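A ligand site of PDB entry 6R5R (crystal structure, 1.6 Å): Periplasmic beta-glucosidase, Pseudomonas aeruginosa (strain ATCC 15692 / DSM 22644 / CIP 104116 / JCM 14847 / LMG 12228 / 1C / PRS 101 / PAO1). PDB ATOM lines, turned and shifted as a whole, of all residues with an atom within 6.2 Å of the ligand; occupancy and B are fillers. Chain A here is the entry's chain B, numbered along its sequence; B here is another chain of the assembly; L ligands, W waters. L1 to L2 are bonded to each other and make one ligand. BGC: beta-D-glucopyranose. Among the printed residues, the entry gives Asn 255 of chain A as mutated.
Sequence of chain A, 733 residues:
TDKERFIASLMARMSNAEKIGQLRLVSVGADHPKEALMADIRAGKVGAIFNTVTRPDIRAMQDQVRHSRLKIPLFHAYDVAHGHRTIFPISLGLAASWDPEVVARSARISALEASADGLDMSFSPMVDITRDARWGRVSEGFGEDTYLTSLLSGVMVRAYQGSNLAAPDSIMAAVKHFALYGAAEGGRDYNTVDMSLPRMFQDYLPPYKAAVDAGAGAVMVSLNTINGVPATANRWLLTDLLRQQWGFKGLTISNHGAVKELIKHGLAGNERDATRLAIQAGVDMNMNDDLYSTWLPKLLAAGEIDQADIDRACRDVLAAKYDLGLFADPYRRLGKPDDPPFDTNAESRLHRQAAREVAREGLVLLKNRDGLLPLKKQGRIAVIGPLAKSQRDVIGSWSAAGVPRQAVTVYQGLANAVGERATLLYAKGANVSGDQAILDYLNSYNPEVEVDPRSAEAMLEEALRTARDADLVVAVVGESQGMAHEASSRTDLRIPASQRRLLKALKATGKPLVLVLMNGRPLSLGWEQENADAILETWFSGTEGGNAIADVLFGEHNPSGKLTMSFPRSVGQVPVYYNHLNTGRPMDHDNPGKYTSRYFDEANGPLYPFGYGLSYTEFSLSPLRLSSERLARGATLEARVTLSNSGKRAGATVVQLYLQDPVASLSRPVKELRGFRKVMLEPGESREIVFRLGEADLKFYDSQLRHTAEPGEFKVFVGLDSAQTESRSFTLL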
ATOM      1  N   PHE A  50     -11.982  27.805 -12.258  1.00  0.00           N
ATOM      2  CA  PHE A  50     -11.012  27.090 -11.387  1.00  0.00           C
ATOM      3  C   PHE A  50     -10.381  25.943 -12.184  1.00  0.00           C
ATOM      4  O   PHE A  50     -10.986  25.453 -13.177  1.00  0.00           O
ATOM      5  CB  PHE A  50     -11.691  26.660 -10.090  1.00  0.00           C
ATOM      6  CG  PHE A  50     -12.761  25.632 -10.177  1.00  0.00           C
ATOM      7  CD1 PHE A  50     -14.039  25.956 -10.617  1.00  0.00           C
ATOM      8  CD2 PHE A  50     -12.511  24.322  -9.805  1.00  0.00           C
ATOM      9  CE1 PHE A  50     -15.059  25.036 -10.657  1.00  0.00           C
ATOM     10  CE2 PHE A  50     -13.519  23.374  -9.913  1.00  0.00           C
ATOM     11  CZ  PHE A  50     -14.783  23.712 -10.330  1.00  0.00           C
ATOM     12  N   ASN A  51      -9.214  25.523 -11.716  1.00  0.00           N
ATOM     13  CA  ASN A  51      -8.437  24.350 -12.236  1.00  0.00           C
ATOM     14  C   ASN A  51      -7.806  24.634 -13.599  1.00  0.00           C
ATOM     15  O   ASN A  51      -7.307  23.640 -14.203  1.00  0.00           O
ATOM     16  CB  ASN A  51      -9.295  23.081 -12.269  1.00  0.00           C
ATOM     17  CG  ASN A  51      -9.549  22.492 -10.887  1.00  0.00           C
ATOM     18  OD1 ASN A  51      -8.895  22.890  -9.939  1.00  0.00           O
ATOM     19  ND2 ASN A  51     -10.508  21.593 -10.802  1.00  0.00           N
ATOM     20  N   ASP A  79      -6.635  25.104  -6.054  1.00  0.00           N
ATOM     21  CA  ASP A  79      -6.462  24.497  -4.706  1.00  0.00           C
ATOM     22  C   ASP A  79      -4.966  24.521  -4.410  1.00  0.00           C
ATOM     23  O   ASP A  79      -4.330  23.484  -4.443  1.00  0.00           O
ATOM     24  CB  ASP A  79      -7.124  23.121  -4.651  1.00  0.00           C
ATOM     25  CG  ASP A  79      -8.638  23.216  -4.561  1.00  0.00           C
ATOM     26  OD1 ASP A  79      -9.100  23.785  -3.559  1.00  0.00           O
ATOM     27  OD2 ASP A  79      -9.345  22.706  -5.470  1.00  0.00           O
ATOM     28  N   PHE A 123      -8.165  28.412  -3.049  1.00  0.00           N
ATOM     29  CA  PHE A 123      -9.139  27.861  -2.078  1.00  0.00           C
ATOM     30  C   PHE A 123      -8.337  27.360  -0.878  1.00  0.00           C
ATOM     31  O   PHE A 123      -8.139  26.155  -0.749  1.00  0.00           O
ATOM     32  CB  PHE A 123      -9.962  26.787  -2.730  1.00  0.00           C
ATOM     33  CG  PHE A 123     -10.736  27.254  -3.924  1.00  0.00           C
ATOM     34  CD1 PHE A 123     -11.483  28.431  -3.887  1.00  0.00           C
ATOM     35  CD2 PHE A 123     -10.768  26.467  -5.051  1.00  0.00           C
ATOM     36  CE1 PHE A 123     -12.179  28.815  -5.027  1.00  0.00           C
ATOM     37  CE2 PHE A 123     -11.491  26.844  -6.166  1.00  0.00           C
ATOM     38  CZ  PHE A 123     -12.204  28.008  -6.130  1.00  0.00           C
ATOM     39  N   ARG A 137      -9.578  14.257   5.678  1.00  0.00           N
ATOM     40  CA  ARG A 137      -9.129  15.652   5.428  1.00  0.00           C
ATOM     41  C   ARG A 137      -8.379  16.259   6.606  1.00  0.00           C
ATOM     42  O   ARG A 137      -8.063  17.439   6.551  1.00  0.00           O
ATOM     43  CB  ARG A 137     -10.323  16.470   4.988  1.00  0.00           C
ATOM     44  CG  ARG A 137     -10.992  15.845   3.782  1.00  0.00           C
ATOM     45  CD  ARG A 137     -12.014  16.769   3.087  1.00  0.00           C
ATOM     46  NE  ARG A 137     -11.263  17.769   2.338  1.00  0.00           N
ATOM     47  CZ  ARG A 137     -11.718  18.418   1.263  1.00  0.00           C
ATOM     48  NH1 ARG A 137     -12.963  18.203   0.838  1.00  0.00           N
ATOM     49  NH2 ARG A 137     -10.904  19.264   0.654  1.00  0.00           N
ATOM     50  N   GLU A 140      -5.280  18.311   5.830  1.00  0.00           N
ATOM     51  CA  GLU A 140      -5.399  19.656   5.241  1.00  0.00           C
ATOM     52  C   GLU A 140      -5.453  20.755   6.290  1.00  0.00           C
ATOM     53  O   GLU A 140      -5.295  21.889   5.894  1.00  0.00           O
ATOM     54  CB  GLU A 140      -6.658  19.775   4.412  1.00  0.00           C
ATOM     55  CG  GLU A 140      -6.588  18.871   3.236  1.00  0.00           C
ATOM     56  CD  GLU A 140      -7.943  18.713   2.589  1.00  0.00           C
ATOM     57  OE1 GLU A 140      -8.572  19.787   2.241  1.00  0.00           O
ATOM     58  OE2 GLU A 140      -8.356  17.533   2.426  1.00  0.00           O
ATOM     59  N   LYS A 176     -11.545  28.203   3.974  1.00  0.00           N
ATOM     60  CA  LYS A 176     -12.518  27.059   3.866  1.00  0.00           C
ATOM     61  C   LYS A 176     -12.350  26.157   5.104  1.00  0.00           C
ATOM     62  O   LYS A 176     -11.331  26.255   5.797  1.00  0.00           O
ATOM     63  CB  LYS A 176     -12.298  26.328   2.564  1.00  0.00           C
ATOM     64  CG  LYS A 176     -11.028  25.469   2.523  1.00  0.00           C
ATOM     65  CD  LYS A 176     -10.720  25.002   1.124  1.00  0.00           C
ATOM     66  CE  LYS A 176      -9.580  24.022   0.987  1.00  0.00           C
ATOM     67  NZ  LYS A 176      -9.358  23.691  -0.425  1.00  0.00           N
ATOM     68  N   HIS A 177     -13.301  25.309   5.417  1.00  0.00           N
ATOM     69  CA  HIS A 177     -14.627  25.140   4.811  1.00  0.00           C
ATOM     70  C   HIS A 177     -15.656  25.657   5.806  1.00  0.00           C
ATOM     71  O   HIS A 177     -15.843  25.058   6.862  1.00  0.00           O
ATOM     72  CB  HIS A 177     -14.909  23.698   4.453  1.00  0.00           C
ATOM     73  CG  HIS A 177     -13.875  23.043   3.602  1.00  0.00           C
ATOM     74  ND1 HIS A 177     -12.754  22.421   4.100  1.00  0.00           N
ATOM     75  CD2 HIS A 177     -13.831  22.896   2.238  1.00  0.00           C
ATOM     76  CE1 HIS A 177     -12.055  21.906   3.078  1.00  0.00           C
ATOM     77  NE2 HIS A 177     -12.694  22.175   1.953  1.00  0.00           N
ATOM     78  N   TYR A 181     -16.739  21.548   9.197  1.00  0.00           N
ATOM     79  CA  TYR A 181     -16.669  20.377   8.290  1.00  0.00           C
ATOM     80  C   TYR A 181     -15.911  19.226   8.951  1.00  0.00           C
ATOM     81  O   TYR A 181     -16.252  18.084   8.741  1.00  0.00           O
ATOM     82  CB  TYR A 181     -16.078  20.906   6.989  1.00  0.00           C
ATOM     83  CG  TYR A 181     -15.884  19.909   5.874  1.00  0.00           C
ATOM     84  CD1 TYR A 181     -16.828  18.971   5.525  1.00  0.00           C
ATOM     85  CD2 TYR A 181     -14.745  20.024   5.065  1.00  0.00           C
ATOM     86  CE1 TYR A 181     -16.607  18.087   4.459  1.00  0.00           C
ATOM     87  CE2 TYR A 181     -14.535  19.196   3.995  1.00  0.00           C
ATOM     88  CZ  TYR A 181     -15.447  18.195   3.697  1.00  0.00           C
ATOM     89  OH  TYR A 181     -15.177  17.336   2.653  1.00  0.00           O
ATOM     90  N   ASP A 189     -16.496  11.420   5.688  1.00  0.00           N
ATOM     91  CA  ASP A 189     -16.535  12.703   5.001  1.00  0.00           C
ATOM     92  C   ASP A 189     -17.967  13.062   4.577  1.00  0.00           C
ATOM     93  O   ASP A 189     -18.797  12.184   4.316  1.00  0.00           O
ATOM     94  CB  ASP A 189     -15.558  12.714   3.839  1.00  0.00           C
ATOM     95  CG  ASP A 189     -15.055  14.107   3.447  1.00  0.00           C
ATOM     96  OD1 ASP A 189     -15.503  15.141   4.029  1.00  0.00           O
ATOM     97  OD2 ASP A 189     -14.149  14.145   2.594  1.00  0.00           O
ATOM     98  N   TYR A 190     -18.228  14.361   4.612  1.00  0.00           N
ATOM     99  CA  TYR A 190     -19.498  14.972   4.204  1.00  0.00           C
ATOM    100  C   TYR A 190     -20.598  14.703   5.228  1.00  0.00           C
ATOM    101  O   TYR A 190     -21.705  15.253   5.059  1.00  0.00           O
ATOM    102  CB  TYR A 190     -19.946  14.409   2.868  1.00  0.00           C
ATOM    103  CG  TYR A 190     -18.882  14.277   1.812  1.00  0.00           C
ATOM    104  CD1 TYR A 190     -18.144  15.384   1.380  1.00  0.00           C
ATOM    105  CD2 TYR A 190     -18.675  13.046   1.234  1.00  0.00           C
ATOM    106  CE1 TYR A 190     -17.188  15.236   0.400  1.00  0.00           C
ATOM    107  CE2 TYR A 190     -17.742  12.880   0.222  1.00  0.00           C
ATOM    108  CZ  TYR A 190     -17.017  13.983  -0.205  1.00  0.00           C
ATOM    109  OH  TYR A 190     -16.112  13.853  -1.259  1.00  0.00           O
ATOM    110  N   MET A 220     -15.160  29.981   1.358  1.00  0.00           N
ATOM    111  CA  MET A 220     -15.741  28.813   0.664  1.00  0.00           C
ATOM    112  C   MET A 220     -16.623  28.083   1.673  1.00  0.00           C
ATOM    113  O   MET A 220     -16.157  27.720   2.751  1.00  0.00           O
ATOM    114  CB  MET A 220     -14.709  27.856   0.091  1.00  0.00           C
ATOM    115  CG  MET A 220     -15.394  26.722  -0.579  1.00  0.00           C
ATOM    116  SD  MET A 220     -14.199  25.550  -1.279  1.00  0.00           S
ATOM    117  CE  MET A 220     -14.039  26.239  -2.933  1.00  0.00           C
ATOM    118  N   LEU A 223     -19.751  21.529   2.841  1.00  0.00           N
ATOM    119  CA  LEU A 223     -20.670  20.529   2.276  1.00  0.00           C
ATOM    120  C   LEU A 223     -21.599  19.927   3.322  1.00  0.00           C
ATOM    121  O   LEU A 223     -22.580  19.327   2.916  1.00  0.00           O
ATOM    122  CB  LEU A 223     -19.853  19.438   1.587  1.00  0.00           C
ATOM    123  CG  LEU A 223     -19.162  19.847   0.287  1.00  0.00           C
ATOM    124  CD1 LEU A 223     -18.144  18.778  -0.132  1.00  0.00           C
ATOM    125  CD2 LEU A 223     -20.214  20.048  -0.791  1.00  0.00           C
ATOM    126  N   ASN A 255     -19.401  25.366  -2.407  1.00  0.00           N
ATOM    127  CA  ASN A 255     -18.573  24.214  -2.711  1.00  0.00           C
ATOM    128  C   ASN A 255     -19.059  23.564  -3.993  1.00  0.00           C
ATOM    129  O   ASN A 255     -20.079  23.967  -4.636  1.00  0.00           O
ATOM    130  CB  ASN A 255     -18.551  23.318  -1.477  1.00  0.00           C
ATOM    131  CG  ASN A 255     -17.190  22.728  -1.219  1.00  0.00           C
ATOM    132  OD1 ASN A 255     -16.637  22.137  -2.133  1.00  0.00           O
ATOM    133  ND2 ASN A 255     -16.660  22.909   0.004  1.00  0.00           N
ATOM    134  N   HIS A 256     -18.390  22.517  -4.358  1.00  0.00           N
ATOM    135  CA  HIS A 256     -18.466  21.937  -5.709  1.00  0.00           C
ATOM    136  C   HIS A 256     -19.773  21.157  -5.883  1.00  0.00           C
ATOM    137  O   HIS A 256     -19.944  20.124  -5.235  1.00  0.00           O
ATOM    138  CB  HIS A 256     -17.237  21.054  -5.850  1.00  0.00           C
ATOM    139  CG  HIS A 256     -17.070  20.626  -7.253  1.00  0.00           C
ATOM    140  ND1 HIS A 256     -17.896  19.694  -7.812  1.00  0.00           N
ATOM    141  CD2 HIS A 256     -16.204  21.031  -8.207  1.00  0.00           C
ATOM    142  CE1 HIS A 256     -17.529  19.507  -9.077  1.00  0.00           C
ATOM    143  NE2 HIS A 256     -16.480  20.308  -9.343  1.00  0.00           N
ATOM    144  N   MET A 287     -20.502  27.152  -7.690  1.00  0.00           N
ATOM    145  CA  MET A 287     -19.402  26.342  -8.243  1.00  0.00           C
ATOM    146  C   MET A 287     -19.971  25.134  -9.012  1.00  0.00           C
ATOM    147  O   MET A 287     -20.620  24.234  -8.409  1.00  0.00           O
ATOM    148  CB  MET A 287     -18.445  25.923  -7.129  1.00  0.00           C
ATOM    149  CG  MET A 287     -17.231  25.222  -7.595  1.00  0.00           C
ATOM    150  SD  MET A 287     -16.149  24.956  -6.108  1.00  0.00           S
ATOM    151  CE  MET A 287     -14.548  24.766  -6.882  1.00  0.00           C
ATOM    152  N   TRP A 398      -3.795  16.910  -2.256  1.00  0.00           N
ATOM    153  CA  TRP A 398      -3.989  18.339  -2.617  1.00  0.00           C
ATOM    154  C   TRP A 398      -2.621  18.958  -2.971  1.00  0.00           C
ATOM    155  O   TRP A 398      -2.222  19.983  -2.417  1.00  0.00           O
ATOM    156  CB  TRP A 398      -4.752  19.079  -1.530  1.00  0.00           C
ATOM    157  CG  TRP A 398      -6.182  18.607  -1.393  1.00  0.00           C
ATOM    158  CD1 TRP A 398      -6.677  17.930  -0.314  1.00  0.00           C
ATOM    159  CD2 TRP A 398      -7.298  18.779  -2.301  1.00  0.00           C
ATOM    160  NE1 TRP A 398      -8.028  17.673  -0.503  1.00  0.00           N
ATOM    161  CE2 TRP A 398      -8.418  18.165  -1.711  1.00  0.00           C
ATOM    162  CE3 TRP A 398      -7.463  19.373  -3.561  1.00  0.00           C
ATOM    163  CZ2 TRP A 398      -9.671  18.117  -2.338  1.00  0.00           C
ATOM    164  CZ3 TRP A 398      -8.687  19.318  -4.183  1.00  0.00           C
ATOM    165  CH2 TRP A 398      -9.786  18.699  -3.582  1.00  0.00           C
ATOM    166  N   HIS A 485      -7.174  11.698   2.293  1.00  0.00           N
ATOM    167  CA  HIS A 485      -7.645  12.661   1.288  1.00  0.00           C
ATOM    168  C   HIS A 485      -9.168  12.810   1.396  1.00  0.00           C
ATOM    169  O   HIS A 485      -9.784  12.149   2.253  1.00  0.00           O
ATOM    170  CB  HIS A 485      -7.041  12.251  -0.063  1.00  0.00           C
ATOM    171  CG  HIS A 485      -7.978  11.944  -1.171  1.00  0.00           C
ATOM    172  ND1 HIS A 485      -8.467  10.676  -1.407  1.00  0.00           N
ATOM    173  CD2 HIS A 485      -8.499  12.742  -2.127  1.00  0.00           C
ATOM    174  CE1 HIS A 485      -9.240  10.728  -2.474  1.00  0.00           C
ATOM    175  NE2 HIS A 485      -9.303  11.972  -2.919  1.00  0.00           N
ATOM    176  N   GLU A 486      -9.727  13.685   0.595  1.00  0.00           N
ATOM    177  CA  GLU A 486     -11.184  13.798   0.551  1.00  0.00           C
ATOM    178  C   GLU A 486     -11.779  12.413   0.417  1.00  0.00           C
ATOM    179  O   GLU A 486     -11.350  11.624  -0.460  1.00  0.00           O
ATOM    180  CB  GLU A 486     -11.537  14.726  -0.598  1.00  0.00           C
ATOM    181  CG  GLU A 486     -13.020  14.843  -0.762  1.00  0.00           C
ATOM    182  CD  GLU A 486     -13.506  15.715  -1.888  1.00  0.00           C
ATOM    183  OE1 GLU A 486     -12.639  16.215  -2.638  1.00  0.00           O
ATOM    184  OE2 GLU A 486     -14.766  15.949  -1.947  1.00  0.00           O
ATOM    185  N   ARG B 586     -23.951  13.683  -0.309  1.00  0.00           N
ATOM    186  CA  ARG B 586     -23.170  12.686  -1.094  1.00  0.00           C
ATOM    187  C   ARG B 586     -23.372  11.321  -0.473  1.00  0.00           C
ATOM    188  O   ARG B 586     -22.413  10.672  -0.059  1.00  0.00           O
ATOM    189  CB  ARG B 586     -21.698  13.096  -1.135  1.00  0.00           C
ATOM    190  CG  ARG B 586     -21.443  14.342  -1.964  1.00  0.00           C
ATOM    191  CD  ARG B 586     -19.992  14.736  -2.087  1.00  0.00           C
ATOM    192  NE  ARG B 586     -19.879  16.022  -2.770  1.00  0.00           N
ATOM    193  CZ  ARG B 586     -18.780  16.532  -3.237  1.00  0.00           C
ATOM    194  NH1 ARG B 586     -17.649  15.847  -3.144  1.00  0.00           N
ATOM    195  NH2 ARG B 586     -18.803  17.690  -3.880  1.00  0.00           N
ATOM    196  N   TYR B 596     -16.546   9.264  -3.990  1.00  0.00           N
ATOM    197  CA  TYR B 596     -16.822  10.606  -3.420  1.00  0.00           C
ATOM    198  C   TYR B 596     -18.178  10.630  -2.747  1.00  0.00           C
ATOM    199  O   TYR B 596     -19.080  11.417  -3.079  1.00  0.00           O
ATOM    200  CB  TYR B 596     -16.572  11.721  -4.432  1.00  0.00           C
ATOM    201  CG  TYR B 596     -15.124  11.841  -4.779  1.00  0.00           C
ATOM    202  CD1 TYR B 596     -14.235  12.497  -3.939  1.00  0.00           C
ATOM    203  CD2 TYR B 596     -14.600  11.212  -5.905  1.00  0.00           C
ATOM    204  CE1 TYR B 596     -12.884  12.607  -4.238  1.00  0.00           C
ATOM    205  CE2 TYR B 596     -13.239  11.278  -6.193  1.00  0.00           C
ATOM    206  CZ  TYR B 596     -12.372  11.975  -5.358  1.00  0.00           C
ATOM    207  OH  TYR B 596     -11.051  12.081  -5.655  1.00  0.00           O
HETATM  208  C2  BGC L   1     -11.798  22.374  -2.829  1.00  0.00           C
HETATM  209  C3  BGC L   1     -12.742  22.274  -4.033  1.00  0.00           C
HETATM  210  C4  BGC L   1     -13.069  20.770  -4.123  1.00  0.00           C
HETATM  211  C5  BGC L   1     -13.810  20.386  -2.833  1.00  0.00           C
HETATM  212  C6  BGC L   1     -14.186  18.909  -2.846  1.00  0.00           C
HETATM  213  C1  BGC L   1     -12.509  21.870  -1.549  1.00  0.00           C
HETATM  214  O1  BGC L   1     -11.598  21.872  -0.533  1.00  0.00           O
HETATM  215  O2  BGC L   1     -11.417  23.727  -2.543  1.00  0.00           O
HETATM  216  O3  BGC L   1     -11.989  22.692  -5.215  1.00  0.00           O
HETATM  217  O4  BGC L   1     -13.946  20.604  -5.234  1.00  0.00           O
HETATM  218  O5  BGC L   1     -12.882  20.505  -1.747  1.00  0.00           O
HETATM  219  O6  BGC L   1     -14.704  18.647  -1.523  1.00  0.00           O
HETATM  220  C2  BGC L   2     -12.174  20.193  -6.947  1.00  0.00           C
HETATM  221  C3  BGC L   2     -11.829  19.199  -8.058  1.00  0.00           C
HETATM  222  C4  BGC L   2     -11.678  17.803  -7.411  1.00  0.00           C
HETATM  223  C5  BGC L   2     -12.973  17.447  -6.654  1.00  0.00           C
HETATM  224  C6  BGC L   2     -12.779  16.133  -5.882  1.00  0.00           C
HETATM  225  C1  BGC L   2     -13.466  19.706  -6.277  1.00  0.00           C
HETATM  226  O2  BGC L   2     -12.394  21.509  -7.494  1.00  0.00           O
HETATM  227  O3  BGC L   2     -10.589  19.630  -8.627  1.00  0.00           O
HETATM  228  O4  BGC L   2     -11.460  16.870  -8.461  1.00  0.00           O
HETATM  229  O5  BGC L   2     -13.246  18.457  -5.625  1.00  0.00           O
HETATM  230  O6  BGC L   2     -14.021  15.855  -5.191  1.00  0.00           O
HETATM  231  O   HOH W   1     -16.333  17.503  -5.354  1.00  0.00           O
HETATM  232  O   HOH W   2     -15.152  20.492   0.474  1.00  0.00           O
HETATM  233  O   HOH W   3      -8.458  21.252  -7.503  1.00  0.00           O
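An oxygen (O2) of BGC L1 is in hydrogen-bond range of the side-chain carboxylate (OD1) of Asp 79 (2.5 Å). The side-chain amide nitrogen (ND2) of Asn 51 sits at hydrogen-bond distance from an oxygen (O3) of BGC L2 (2.9 Å). The side-chain amino group (NZ) of Lys 176 lies within hydrogen-bond range of an oxygen (O1) of BGC L1 (2.9 Å). An oxygen (O1) of BGC L1 lies within hydrogen-bond range of a ring nitrogen (NE2) of His 177 (2.7 Å). The side-chain sulfur (SD) of Met 220 lies within hydrogen-bond range of an oxygen (O2) of BGC L1 (3.6 Å). The guanidinium group (NH2) of Arg 137 is in hydrogen-bond range of an oxygen (O1) of BGC L1. An oxygen (O6) of BGC L1 lies within hydrogen-bond range of the side-chain carboxylate of Glu 486.
OD1 of Asp 79 is in salt-bridge range of NZ of Lys 176 (3.1 Å). SD of Met 287 lies within hydrogen-bond range of N of His 256. The guanidinium group (NH2) of Arg 586 of chain B is in hydrogen-bond range of the backbone carbonyl oxygen (O) of His 256, at 3.0 Å. The indole nitrogen (NE1) of Trp 398 is in hydrogen-bond range of the side-chain carboxylate (OE2) of Glu 140 (3.0 Å). The side-chain carboxylate of Glu 486 lies within hydrogen-bond range of the side-chain hydroxyl of Tyr 190 (2.6 Å). The side-chain carboxylate of Glu 140 is in salt-bridge range of the guanidinium group of Arg 137, at 2.9 Å. The side-chain carboxylate (OE2) of Glu 486 lies within salt-bridge range of the guanidinium group (NH1) of Arg 586 of chain B (3.1 Å). The guanidinium group (NH1) of Arg 137 sits at hydrogen-bond distance from the side-chain hydroxyl (OH) of Tyr 181.
Phe 50 touches the ligand. CB of Phe 123 touches O2 of BGC L1, 3.4 Å away. CD1 of Leu 223 touches O6 of BGC L1, 3.7 Å away. OD1 of Asn 255 touches C5 of BGC L1, at 3.4 Å. His 256 touches the ligand. CE of Met 287 touches O3 of BGC L1, at 3.7 Å. CH2 of Trp 398 touches C4 of BGC L1 (3.9 Å). Tyr 596 of chain B touches the ligand. Of the 21 residues printed, 15 come within 4 Å of the ligand. The nearest printed residue that does not touch the ligand is Arg 586 of chain B (4.2 Å).
Water W2 lies within hydrogen-bond range of O6 of BGC L1 (2.8 Å), ND2 of Asn 255 (2.9 Å), NH1 of Arg 137 (3.2 Å) and NE2 of His 177 (3.3 Å). Water W1 bridges O6 of BGC L2 (2.8 Å) and NH2 of Arg 586 of chain B (2.9 Å). Water W3 lies within hydrogen-bond range of OD2 of Asp 79 (2.7 Å), O3 of BGC L2 (2.9 Å) and OD1 of Asn 51 (3.0 Å).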
